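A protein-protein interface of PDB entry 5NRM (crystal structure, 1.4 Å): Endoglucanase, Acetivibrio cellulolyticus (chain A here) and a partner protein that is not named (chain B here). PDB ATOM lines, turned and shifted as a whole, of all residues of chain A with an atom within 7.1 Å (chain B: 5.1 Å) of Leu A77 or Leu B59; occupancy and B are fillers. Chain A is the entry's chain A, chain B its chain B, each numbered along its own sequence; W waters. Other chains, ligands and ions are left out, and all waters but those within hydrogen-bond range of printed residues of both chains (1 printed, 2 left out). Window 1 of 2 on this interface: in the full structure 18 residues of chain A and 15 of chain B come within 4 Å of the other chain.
Of the 20 printed residues of chain A, 11 touch a printed residue of chain B.
Printed residues of chain A that touch a printed residue of chain B: Thr A34, Ala A35, Asp A36, Phe A64, Gly A65, Asn A67, Glu A69, Lys A75, Leu A77, Leu A79 and Tyr A81.
Printed residues of chain B that touch a printed residue of chain A: Asn B12, Ser B13, Phe B16, Arg B56, Leu B59, Leu B60 and Gly B61.
Among the printed residues, no Asp or Glu carboxylate lies within 4 Å of a Lys or Arg side-chain nitrogen of the other chain.
Among the printed residues, pairs that only touch across the chains: Asp A36 with Asn B12, Gly A65 with Arg B56, Gly A65 with Leu B60, Glu A69 with Gly B61, Lys A75 with Leu B59, Lys A75 with Leu B60, Lys A75 with Gly B61, Leu A77 with Phe B16, Leu A77 with Arg B56, Leu A77 with Leu B59, Leu A77 with Leu B60, Leu A79 with Phe B16 and Tyr A81 with Phe B16.
The backbone NH (N) of Ala A35 is in hydrogen-bond range of the backbone carbonyl oxygen (O) of Phe A78 (2.9 Å).
OG1 of Thr A38 lies within hydrogen-bond range of NZ of Lys A75 (2.9 Å).
The side-chain amide oxygen (OD1) of Asn A63 sits at hydrogen-bond distance from the backbone NH (N) of Tyr A81 (3.1 Å).
The backbone carbonyl oxygen (O) of Leu A77 lies within hydrogen-bond range of the backbone NH (N) of Gly A65 (2.8 Å).
The backbone carbonyl oxygen of Asn A67 sits at hydrogen-bond distance from the backbone NH of Lys A75, 2.9 Å away.
The side-chain sulfur (SD) of Met B55 lies within hydrogen-bond range of the backbone NH (N) of Phe B16, at 3.4 Å.
The side-chain hydroxyl (OG) of Ser B13 lies within hydrogen-bond range of the side-chain hydroxyl (OG1) of Thr A34, 2.9 Å away.
N of Ala A35 lies close to OG of Ser B13, 3.4 Å away.
OD1 of Asp A36 sits at hydrogen-bond distance from OG of Ser B13.
The backbone carbonyl oxygen (O) of Phe A64 sits at hydrogen-bond distance from the guanidinium group (NH2) of Arg B56 (3.2 Å).
The side-chain amide nitrogen of Asn A67 lies within hydrogen-bond range of the backbone carbonyl oxygen of Leu B60 (2.9 Å).
The side-chain hydroxyl of Tyr A81 lies within hydrogen-bond range of the guanidinium group of Arg B56 (3.2 Å).
Printed residues of chain B within 4 Å of Leu A77: Phe B16, Arg B56, Leu B59 and Leu B60.
Of the printed residues of chain A, Leu B59 touches Lys A75 and Leu A77.
Of the printed residues of chain B, Thr A34 touches Ser B13 (2.9 Å).
Of the printed residues of chain B, Gly A65 touches Arg B56 and Leu B60.
Tyr B58 touches none of the printed residues of chain A.
Val A57 touches none of the printed residues of chain B.
The nearest residue of chain B that does not touch Leu A77 is Ser B13 (4.1 Å).
Water W1 bridges the side-chain carboxylate (OD2) of Asp A36 and the backbone carbonyl oxygen (O) of Ile B11.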
ATOM      1  N   THR A  34     -22.985   0.664 -28.922  1.00  0.00           N
ATOM      2  CA  THR A  34     -23.072   0.253 -27.503  1.00  0.00           C
ATOM      3  C   THR A  34     -21.684   0.117 -26.917  1.00  0.00           C
ATOM      4  O   THR A  34     -20.732  -0.279 -27.645  1.00  0.00           O
ATOM      5  CB  THR A  34     -23.812  -1.149 -27.319  1.00  0.00           C
ATOM      6  OG1 THR A  34     -22.876  -2.244 -27.324  1.00  0.00           O
ATOM      7  CG2 THR A  34     -24.743  -1.484 -28.397  1.00  0.00           C
ATOM      8  N   ALA A  35     -21.543   0.348 -25.629  1.00  0.00           N
ATOM      9  CA  ALA A  35     -20.275   0.074 -24.931  1.00  0.00           C
ATOM     10  C   ALA A  35     -20.527  -0.201 -23.500  1.00  0.00           C
ATOM     11  O   ALA A  35     -21.383   0.483 -22.892  1.00  0.00           O
ATOM     12  CB  ALA A  35     -19.305   1.226 -25.077  1.00  0.00           C
ATOM     13  N   ASP A  36     -19.744  -1.118 -22.894  1.00  0.00           N
ATOM     14  CA  ASP A  36     -19.685  -1.247 -21.463  1.00  0.00           C
ATOM     15  C   ASP A  36     -18.346  -1.732 -21.055  1.00  0.00           C
ATOM     16  O   ASP A  36     -17.829  -2.676 -21.620  1.00  0.00           O
ATOM     17  CB  ASP A  36     -20.824  -2.136 -20.861  1.00  0.00           C
ATOM     18  CG  ASP A  36     -20.668  -3.611 -21.190  1.00  0.00           C
ATOM     19  OD1 ASP A  36     -20.996  -3.917 -22.324  1.00  0.00           O
ATOM     20  OD2 ASP A  36     -20.209  -4.390 -20.333  1.00  0.00           O
ATOM     21  N   PHE A  37     -17.831  -1.159 -19.995  1.00  0.00           N
ATOM     22  CA  PHE A  37     -16.532  -1.630 -19.461  1.00  0.00           C
ATOM     23  C   PHE A  37     -16.324  -1.066 -18.082  1.00  0.00           C
ATOM     24  O   PHE A  37     -17.043  -0.146 -17.668  1.00  0.00           O
ATOM     25  CB  PHE A  37     -15.342  -1.339 -20.393  1.00  0.00           C
ATOM     26  CG  PHE A  37     -15.148   0.110 -20.746  1.00  0.00           C
ATOM     27  CD1 PHE A  37     -14.465   0.998 -19.952  1.00  0.00           C
ATOM     28  CD2 PHE A  37     -15.718   0.621 -21.923  1.00  0.00           C
ATOM     29  CE1 PHE A  37     -14.278   2.312 -20.337  1.00  0.00           C
ATOM     30  CE2 PHE A  37     -15.525   1.907 -22.336  1.00  0.00           C
ATOM     31  CZ  PHE A  37     -14.819   2.780 -21.522  1.00  0.00           C
ATOM     32  N   THR A  38     -15.375  -1.709 -17.390  1.00  0.00           N
ATOM     33  CA  THR A  38     -15.005  -1.325 -16.036  1.00  0.00           C
ATOM     34  C   THR A  38     -13.651  -0.646 -16.139  1.00  0.00           C
ATOM     35  O   THR A  38     -12.768  -1.105 -16.832  1.00  0.00           O
ATOM     36  CB  THR A  38     -14.874  -2.543 -15.151  1.00  0.00           C
ATOM     37  OG1 THR A  38     -16.120  -3.205 -15.032  1.00  0.00           O
ATOM     38  CG2 THR A  38     -14.415  -2.213 -13.714  1.00  0.00           C
ATOM     39  N   VAL A  57     -18.950  11.322 -28.070  1.00  0.00           N
ATOM     40  CA  VAL A  57     -20.161  10.723 -27.632  1.00  0.00           C
ATOM     41  C   VAL A  57     -21.402  11.490 -28.094  1.00  0.00           C
ATOM     42  O   VAL A  57     -21.542  12.693 -27.906  1.00  0.00           O
ATOM     43  CB  VAL A  57     -20.135  10.526 -26.082  1.00  0.00           C
ATOM     44  CG1 VAL A  57     -21.468   9.973 -25.504  1.00  0.00           C
ATOM     45  CG2 VAL A  57     -18.978   9.637 -25.660  1.00  0.00           C
ATOM     46  N   ASN A  63     -27.452   9.117 -23.543  1.00  0.00           N
ATOM     47  CA  ASN A  63     -26.832   7.868 -24.003  1.00  0.00           C
ATOM     48  C   ASN A  63     -25.740   7.361 -23.141  1.00  0.00           C
ATOM     49  O   ASN A  63     -25.339   6.207 -23.288  1.00  0.00           O
ATOM     50  CB  ASN A  63     -26.221   8.110 -25.379  1.00  0.00           C
ATOM     51  CG  ASN A  63     -27.264   8.289 -26.489  1.00  0.00           C
ATOM     52  OD1 ASN A  63     -28.464   8.020 -26.305  1.00  0.00           O
ATOM     53  ND2 ASN A  63     -26.785   8.636 -27.649  1.00  0.00           N
ATOM     54  N   PHE A  64     -25.193   8.180 -22.260  1.00  0.00           N
ATOM     55  CA  PHE A  64     -23.943   7.857 -21.587  1.00  0.00           C
ATOM     56  C   PHE A  64     -24.031   7.907 -20.103  1.00  0.00           C
ATOM     57  O   PHE A  64     -24.560   8.907 -19.532  1.00  0.00           O
ATOM     58  CB  PHE A  64     -22.898   8.877 -22.077  1.00  0.00           C
ATOM     59  CG  PHE A  64     -21.494   8.663 -21.540  1.00  0.00           C
ATOM     60  CD1 PHE A  64     -20.521   7.949 -22.267  1.00  0.00           C
ATOM     61  CD2 PHE A  64     -21.099   9.294 -20.337  1.00  0.00           C
ATOM     62  CE1 PHE A  64     -19.243   7.813 -21.777  1.00  0.00           C
ATOM     63  CE2 PHE A  64     -19.798   9.116 -19.855  1.00  0.00           C
ATOM     64  CZ  PHE A  64     -18.907   8.386 -20.572  1.00  0.00           C
ATOM     65  N   GLY A  65     -23.410   6.976 -19.439  1.00  0.00           N
ATOM     66  CA  GLY A  65     -23.286   7.042 -18.004  1.00  0.00           C
ATOM     67  C   GLY A  65     -21.963   6.494 -17.496  1.00  0.00           C
ATOM     68  O   GLY A  65     -21.401   5.544 -18.056  1.00  0.00           O
ATOM     69  N   ILE A  66     -21.519   7.024 -16.339  1.00  0.00           N
ATOM     70  CA  ILE A  66     -20.386   6.518 -15.602  1.00  0.00           C
ATOM     71  C   ILE A  66     -20.738   6.542 -14.125  1.00  0.00           C
ATOM     72  O   ILE A  66     -21.283   7.562 -13.629  1.00  0.00           O
ATOM     73  CB  ILE A  66     -19.093   7.303 -15.982  1.00  0.00           C
ATOM     74  CG1 ILE A  66     -17.855   6.601 -15.420  1.00  0.00           C
ATOM     75  CG2 ILE A  66     -19.215   8.772 -15.618  1.00  0.00           C
ATOM     76  CD1 ILE A  66     -16.555   7.046 -16.069  1.00  0.00           C
ATOM     77  N   ASN A  67     -20.463   5.474 -13.399  1.00  0.00           N
ATOM     78  CA  ASN A  67     -20.769   5.405 -11.974  1.00  0.00           C
ATOM     79  C   ASN A  67     -19.595   4.815 -11.214  1.00  0.00           C
ATOM     80  O   ASN A  67     -18.957   3.863 -11.664  1.00  0.00           O
ATOM     81  CB  ASN A  67     -22.013   4.556 -11.763  1.00  0.00           C
ATOM     82  CG  ASN A  67     -22.394   4.424 -10.309  1.00  0.00           C
ATOM     83  OD1 ASN A  67     -22.600   5.430  -9.642  1.00  0.00           O
ATOM     84  ND2 ASN A  67     -22.482   3.223  -9.823  1.00  0.00           N
ATOM     85  N   GLU A  69     -18.647   2.454  -8.692  1.00  0.00           N
ATOM     86  CA  GLU A  69     -19.295   1.319  -8.008  1.00  0.00           C
ATOM     87  C   GLU A  69     -18.724   1.184  -6.570  1.00  0.00           C
ATOM     88  O   GLU A  69     -19.442   0.919  -5.579  1.00  0.00           O
ATOM     89  CB  GLU A  69     -19.120   0.013  -8.785  1.00  0.00           C
ATOM     90  CG  GLU A  69     -19.628  -1.205  -8.033  1.00  0.00           C
ATOM     91  CD  GLU A  69     -19.489  -2.461  -8.864  1.00  0.00           C
ATOM     92  OE1 GLU A  69     -19.658  -2.329 -10.061  1.00  0.00           O
ATOM     93  OE2 GLU A  69     -19.171  -3.534  -8.291  1.00  0.00           O
ATOM     94  N   LEU A  74     -14.892   1.933 -11.447  1.00  0.00           N
ATOM     95  CA  LEU A  74     -15.879   2.645 -12.234  1.00  0.00           C
ATOM     96  C   LEU A  74     -16.527   1.697 -13.248  1.00  0.00           C
ATOM     97  O   LEU A  74     -15.849   0.823 -13.797  1.00  0.00           O
ATOM     98  CB  LEU A  74     -15.252   3.818 -12.984  1.00  0.00           C
ATOM     99  CG  LEU A  74     -14.372   4.777 -12.190  1.00  0.00           C
ATOM    100  CD1 LEU A  74     -13.739   5.819 -13.073  1.00  0.00           C
ATOM    101  CD2 LEU A  74     -15.150   5.407 -11.011  1.00  0.00           C
ATOM    102  N   LYS A  75     -17.814   1.967 -13.512  1.00  0.00           N
ATOM    103  CA  LYS A  75     -18.560   1.274 -14.570  1.00  0.00           C
ATOM    104  C   LYS A  75     -18.942   2.318 -15.601  1.00  0.00           C
ATOM    105  O   LYS A  75     -19.416   3.415 -15.214  1.00  0.00           O
ATOM    106  CB  LYS A  75     -19.809   0.608 -13.973  1.00  0.00           C
ATOM    107  CG  LYS A  75     -19.564  -0.233 -12.733  1.00  0.00           C
ATOM    108  CD  LYS A  75     -18.678  -1.438 -12.968  1.00  0.00           C
ATOM    109  CE  LYS A  75     -19.246  -2.382 -14.004  1.00  0.00           C
ATOM    110  NZ  LYS A  75     -18.769  -3.789 -13.954  1.00  0.00           N
ATOM    111  N   VAL A  76     -18.760   1.996 -16.885  1.00  0.00           N
ATOM    112  CA  VAL A  76     -18.965   2.914 -17.960  1.00  0.00           C
ATOM    113  C   VAL A  76     -19.995   2.299 -18.892  1.00  0.00           C
ATOM    114  O   VAL A  76     -19.910   1.090 -19.172  1.00  0.00           O
ATOM    115  CB  VAL A  76     -17.707   3.238 -18.704  1.00  0.00           C
ATOM    116  CG1 VAL A  76     -17.956   4.306 -19.767  1.00  0.00           C
ATOM    117  CG2 VAL A  76     -16.654   3.801 -17.710  1.00  0.00           C
ATOM    118  N   LEU A  77     -20.968   3.068 -19.407  1.00  0.00           N
ATOM    119  CA  LEU A  77     -22.000   2.531 -20.259  1.00  0.00           C
ATOM    120  C   LEU A  77     -22.342   3.564 -21.338  1.00  0.00           C
ATOM    121  O   LEU A  77     -22.573   4.755 -21.014  1.00  0.00           O
ATOM    122  CB  LEU A  77     -23.273   2.266 -19.421  1.00  0.00           C
ATOM    123  CG  LEU A  77     -24.481   1.730 -20.208  1.00  0.00           C
ATOM    124  CD1 LEU A  77     -24.233   0.359 -20.738  1.00  0.00           C
ATOM    125  CD2 LEU A  77     -25.642   1.626 -19.234  1.00  0.00           C
ATOM    126  N   PHE A  78     -22.529   3.128 -22.571  1.00  0.00           N
ATOM    127  CA  PHE A  78     -23.019   3.946 -23.667  1.00  0.00           C
ATOM    128  C   PHE A  78     -24.025   3.129 -24.497  1.00  0.00           C
ATOM    129  O   PHE A  78     -23.801   1.937 -24.770  1.00  0.00           O
ATOM    130  CB  PHE A  78     -21.880   4.416 -24.612  1.00  0.00           C
ATOM    131  CG  PHE A  78     -22.343   5.036 -25.885  1.00  0.00           C
ATOM    132  CD1 PHE A  78     -22.830   6.382 -25.954  1.00  0.00           C
ATOM    133  CD2 PHE A  78     -22.399   4.283 -27.029  1.00  0.00           C
ATOM    134  CE1 PHE A  78     -23.299   6.897 -27.134  1.00  0.00           C
ATOM    135  CE2 PHE A  78     -22.856   4.807 -28.254  1.00  0.00           C
ATOM    136  CZ  PHE A  78     -23.352   6.111 -28.303  1.00  0.00           C
ATOM    137  N   LEU A  79     -25.108   3.776 -24.948  1.00  0.00           N
ATOM    138  CA  LEU A  79     -25.963   3.221 -25.972  1.00  0.00           C
ATOM    139  C   LEU A  79     -26.551   4.330 -26.798  1.00  0.00           C
ATOM    140  O   LEU A  79     -26.998   5.351 -26.232  1.00  0.00           O
ATOM    141  CB  LEU A  79     -27.118   2.470 -25.236  1.00  0.00           C
ATOM    142  CG  LEU A  79     -28.186   1.838 -26.165  1.00  0.00           C
ATOM    143  CD1 LEU A  79     -27.618   0.704 -27.033  1.00  0.00           C
ATOM    144  CD2 LEU A  79     -29.391   1.372 -25.391  1.00  0.00           C
ATOM    145  N   TYR A  81     -29.524   5.492 -27.829  1.00  0.00           N
ATOM    146  CA  TYR A  81     -30.918   5.185 -27.445  1.00  0.00           C
ATOM    147  C   TYR A  81     -31.822   5.264 -28.678  1.00  0.00           C
ATOM    148  O   TYR A  81     -32.887   4.639 -28.629  1.00  0.00           O
ATOM    149  CB  TYR A  81     -31.442   6.182 -26.413  1.00  0.00           C
ATOM    150  CG  TYR A  81     -31.181   5.781 -24.976  1.00  0.00           C
ATOM    151  CD1 TYR A  81     -29.940   5.280 -24.569  1.00  0.00           C
ATOM    152  CD2 TYR A  81     -32.159   5.862 -24.035  1.00  0.00           C
ATOM    153  CE1 TYR A  81     -29.701   4.943 -23.255  1.00  0.00           C
ATOM    154  CE2 TYR A  81     -31.908   5.557 -22.701  1.00  0.00           C
ATOM    155  CZ  TYR A  81     -30.692   5.078 -22.319  1.00  0.00           C
ATOM    156  OH  TYR A  81     -30.364   4.733 -21.021  1.00  0.00           O
ATOM    157  N   PHE A  94     -13.545   9.322 -25.538  1.00  0.00           N
ATOM    158  CA  PHE A  94     -14.835   8.721 -25.153  1.00  0.00           C
ATOM    159  C   PHE A  94     -15.288   9.070 -23.741  1.00  0.00           C
ATOM    160  O   PHE A  94     -16.478   9.203 -23.482  1.00  0.00           O
ATOM    161  CB  PHE A  94     -14.697   7.167 -25.286  1.00  0.00           C
ATOM    162  CG  PHE A  94     -15.959   6.396 -24.914  1.00  0.00           C
ATOM    163  CD1 PHE A  94     -17.047   6.329 -25.794  1.00  0.00           C
ATOM    164  CD2 PHE A  94     -16.022   5.705 -23.770  1.00  0.00           C
ATOM    165  CE1 PHE A  94     -18.149   5.572 -25.423  1.00  0.00           C
ATOM    166  CE2 PHE A  94     -17.140   4.989 -23.383  1.00  0.00           C
ATOM    167  CZ  PHE A  94     -18.182   4.874 -24.230  1.00  0.00           C
ATOM    168  N   ILE B  11     -24.017 -10.639 -19.331  1.00  0.00           N
ATOM    169  CA  ILE B  11     -24.972  -9.520 -19.426  1.00  0.00           C
ATOM    170  C   ILE B  11     -24.150  -8.281 -19.765  1.00  0.00           C
ATOM    171  O   ILE B  11     -23.263  -7.875 -18.981  1.00  0.00           O
ATOM    172  CB  ILE B  11     -25.704  -9.328 -18.069  1.00  0.00           C
ATOM    173  CG1 ILE B  11     -26.526 -10.589 -17.681  1.00  0.00           C
ATOM    174  CG2 ILE B  11     -26.584  -8.086 -18.185  1.00  0.00           C
ATOM    175  CD1 ILE B  11     -26.834 -10.596 -16.230  1.00  0.00           C
ATOM    176  N   ASN B  12     -24.422  -7.647 -20.901  1.00  0.00           N
ATOM    177  CA  ASN B  12     -23.599  -6.538 -21.332  1.00  0.00           C
ATOM    178  C   ASN B  12     -24.411  -5.551 -22.179  1.00  0.00           C
ATOM    179  O   ASN B  12     -25.644  -5.635 -22.244  1.00  0.00           O
ATOM    180  CB  ASN B  12     -22.319  -7.056 -22.036  1.00  0.00           C
ATOM    181  CG  ASN B  12     -22.602  -7.802 -23.352  1.00  0.00           C
ATOM    182  OD1 ASN B  12     -23.568  -7.496 -24.049  1.00  0.00           O
ATOM    183  ND2 ASN B  12     -21.712  -8.731 -23.693  1.00  0.00           N
ATOM    184  N   SER B  13     -23.708  -4.572 -22.744  1.00  0.00           N
ATOM    185  CA  SER B  13     -24.393  -3.489 -23.419  1.00  0.00           C
ATOM    186  C   SER B  13     -25.063  -3.907 -24.743  1.00  0.00           C
ATOM    187  O   SER B  13     -25.956  -3.210 -25.239  1.00  0.00           O
ATOM    188  CB  SER B  13     -23.411  -2.322 -23.687  1.00  0.00           C
ATOM    189  OG  SER B  13     -22.307  -2.743 -24.501  1.00  0.00           O
ATOM    190  N   PHE B  16     -28.375  -4.846 -23.466  1.00  0.00           N
ATOM    191  CA  PHE B  16     -29.090  -3.584 -23.262  1.00  0.00           C
ATOM    192  C   PHE B  16     -29.633  -2.995 -24.552  1.00  0.00           C
ATOM    193  O   PHE B  16     -30.756  -2.534 -24.592  1.00  0.00           O
ATOM    194  CB  PHE B  16     -28.068  -2.645 -22.634  1.00  0.00           C
ATOM    195  CG  PHE B  16     -28.557  -1.314 -22.075  1.00  0.00           C
ATOM    196  CD1 PHE B  16     -29.589  -1.247 -21.199  1.00  0.00           C
ATOM    197  CD2 PHE B  16     -27.873  -0.175 -22.371  1.00  0.00           C
ATOM    198  CE1 PHE B  16     -29.945  -0.038 -20.634  1.00  0.00           C
ATOM    199  CE2 PHE B  16     -28.246   1.064 -21.820  1.00  0.00           C
ATOM    200  CZ  PHE B  16     -29.303   1.115 -20.955  1.00  0.00           C
ATOM    201  N   MET B  55     -31.718  -2.805 -16.120  1.00  0.00           N
ATOM    202  CA  MET B  55     -30.495  -3.312 -16.734  1.00  0.00           C
ATOM    203  C   MET B  55     -29.436  -2.215 -16.699  1.00  0.00           C
ATOM    204  O   MET B  55     -28.224  -2.531 -16.483  1.00  0.00           O
ATOM    205  CB  MET B  55     -30.639  -3.928 -18.152  1.00  0.00           C
ATOM    206  CG  MET B  55     -29.295  -4.764 -18.613  1.00  0.00           C
ATOM    207  SD  MET B  55     -29.620  -5.259 -20.310  1.00  0.00           S
ATOM    208  CE  MET B  55     -30.336  -6.851 -19.740  1.00  0.00           C
ATOM    209  N   ARG B  56     -29.834  -0.958 -16.959  1.00  0.00           N
ATOM    210  CA  ARG B  56     -28.874   0.163 -16.934  1.00  0.00           C
ATOM    211  C   ARG B  56     -28.246   0.252 -15.531  1.00  0.00           C
ATOM    212  O   ARG B  56     -27.031   0.364 -15.412  1.00  0.00           O
ATOM    213  CB  ARG B  56     -29.509   1.529 -17.339  1.00  0.00           C
ATOM    214  CG  ARG B  56     -28.531   2.745 -17.233  1.00  0.00           C
ATOM    215  CD  ARG B  56     -29.119   4.033 -17.885  1.00  0.00           C
ATOM    216  NE  ARG B  56     -28.299   5.287 -17.721  1.00  0.00           N
ATOM    217  CZ  ARG B  56     -27.513   5.837 -18.690  1.00  0.00           C
ATOM    218  NH1 ARG B  56     -27.406   5.285 -19.950  1.00  0.00           N
ATOM    219  NH2 ARG B  56     -26.826   6.899 -18.425  1.00  0.00           N
ATOM    220  N   MET B  57     -29.052   0.154 -14.487  1.00  0.00           N
ATOM    221  CA  MET B  57     -28.525   0.209 -13.105  1.00  0.00           C
ATOM    222  C   MET B  57     -27.544  -0.927 -12.875  1.00  0.00           C
ATOM    223  O   MET B  57     -26.507  -0.740 -12.267  1.00  0.00           O
ATOM    224  CB  MET B  57     -29.621   0.095 -12.075  1.00  0.00           C
ATOM    225  CG  MET B  57     -30.519   1.292 -12.051  1.00  0.00           C
ATOM    226  SD  MET B  57     -32.056   0.978 -11.086  1.00  0.00           S
ATOM    227  CE  MET B  57     -31.488   0.164  -9.586  1.00  0.00           C
ATOM    228  N   TYR B  58     -27.842  -2.124 -13.381  1.00  0.00           N
ATOM    229  CA  TYR B  58     -26.934  -3.265 -13.219  1.00  0.00           C
ATOM    230  C   TYR B  58     -25.594  -3.044 -13.933  1.00  0.00           C
ATOM    231  O   TYR B  58     -24.490  -3.303 -13.384  1.00  0.00           O
ATOM    232  CB  TYR B  58     -27.603  -4.592 -13.695  1.00  0.00           C
ATOM    233  CG  TYR B  58     -26.704  -5.774 -13.714  1.00  0.00           C
ATOM    234  CD1 TYR B  58     -26.510  -6.539 -12.574  1.00  0.00           C
ATOM    235  CD2 TYR B  58     -26.022  -6.120 -14.866  1.00  0.00           C
ATOM    236  CE1 TYR B  58     -25.654  -7.632 -12.605  1.00  0.00           C
ATOM    237  CE2 TYR B  58     -25.174  -7.202 -14.889  1.00  0.00           C
ATOM    238  CZ  TYR B  58     -25.020  -7.944 -13.740  1.00  0.00           C
ATOM    239  OH  TYR B  58     -24.115  -8.978 -13.840  1.00  0.00           O
ATOM    240  N   LEU B  59     -25.675  -2.566 -15.170  1.00  0.00           N
ATOM    241  CA  LEU B  59     -24.470  -2.365 -15.956  1.00  0.00           C
ATOM    242  C   LEU B  59     -23.631  -1.232 -15.379  1.00  0.00           C
ATOM    243  O   LEU B  59     -22.401  -1.249 -15.582  1.00  0.00           O
ATOM    244  CB  LEU B  59     -24.856  -2.055 -17.405  1.00  0.00           C
ATOM    245  CG  LEU B  59     -25.409  -3.296 -18.117  1.00  0.00           C
ATOM    246  CD1 LEU B  59     -25.951  -2.910 -19.513  1.00  0.00           C
ATOM    247  CD2 LEU B  59     -24.376  -4.433 -18.228  1.00  0.00           C
ATOM    248  N   LEU B  60     -24.266  -0.295 -14.693  1.00  0.00           N
ATOM    249  CA  LEU B  60     -23.548   0.768 -13.987  1.00  0.00           C
ATOM    250  C   LEU B  60     -23.045   0.396 -12.570  1.00  0.00           C
ATOM    251  O   LEU B  60     -22.530   1.234 -11.871  1.00  0.00           O
ATOM    252  CB  LEU B  60     -24.331   2.093 -13.953  1.00  0.00           C
ATOM    253  CG  LEU B  60     -24.445   2.778 -15.322  1.00  0.00           C
ATOM    254  CD1 LEU B  60     -25.479   3.892 -15.309  1.00  0.00           C
ATOM    255  CD2 LEU B  60     -23.090   3.205 -15.811  1.00  0.00           C
ATOM    256  N   GLY B  61     -23.267  -0.844 -12.150  1.00  0.00           N
ATOM    257  CA  GLY B  61     -22.886  -1.295 -10.837  1.00  0.00           C
ATOM    258  C   GLY B  61     -23.651  -0.688  -9.668  1.00  0.00           C
ATOM    259  O   GLY B  61     -23.175  -0.652  -8.512  1.00  0.00           O
HETATM  260  O   HOH W   1     -20.974  -6.321 -18.572  1.00  0.00           O
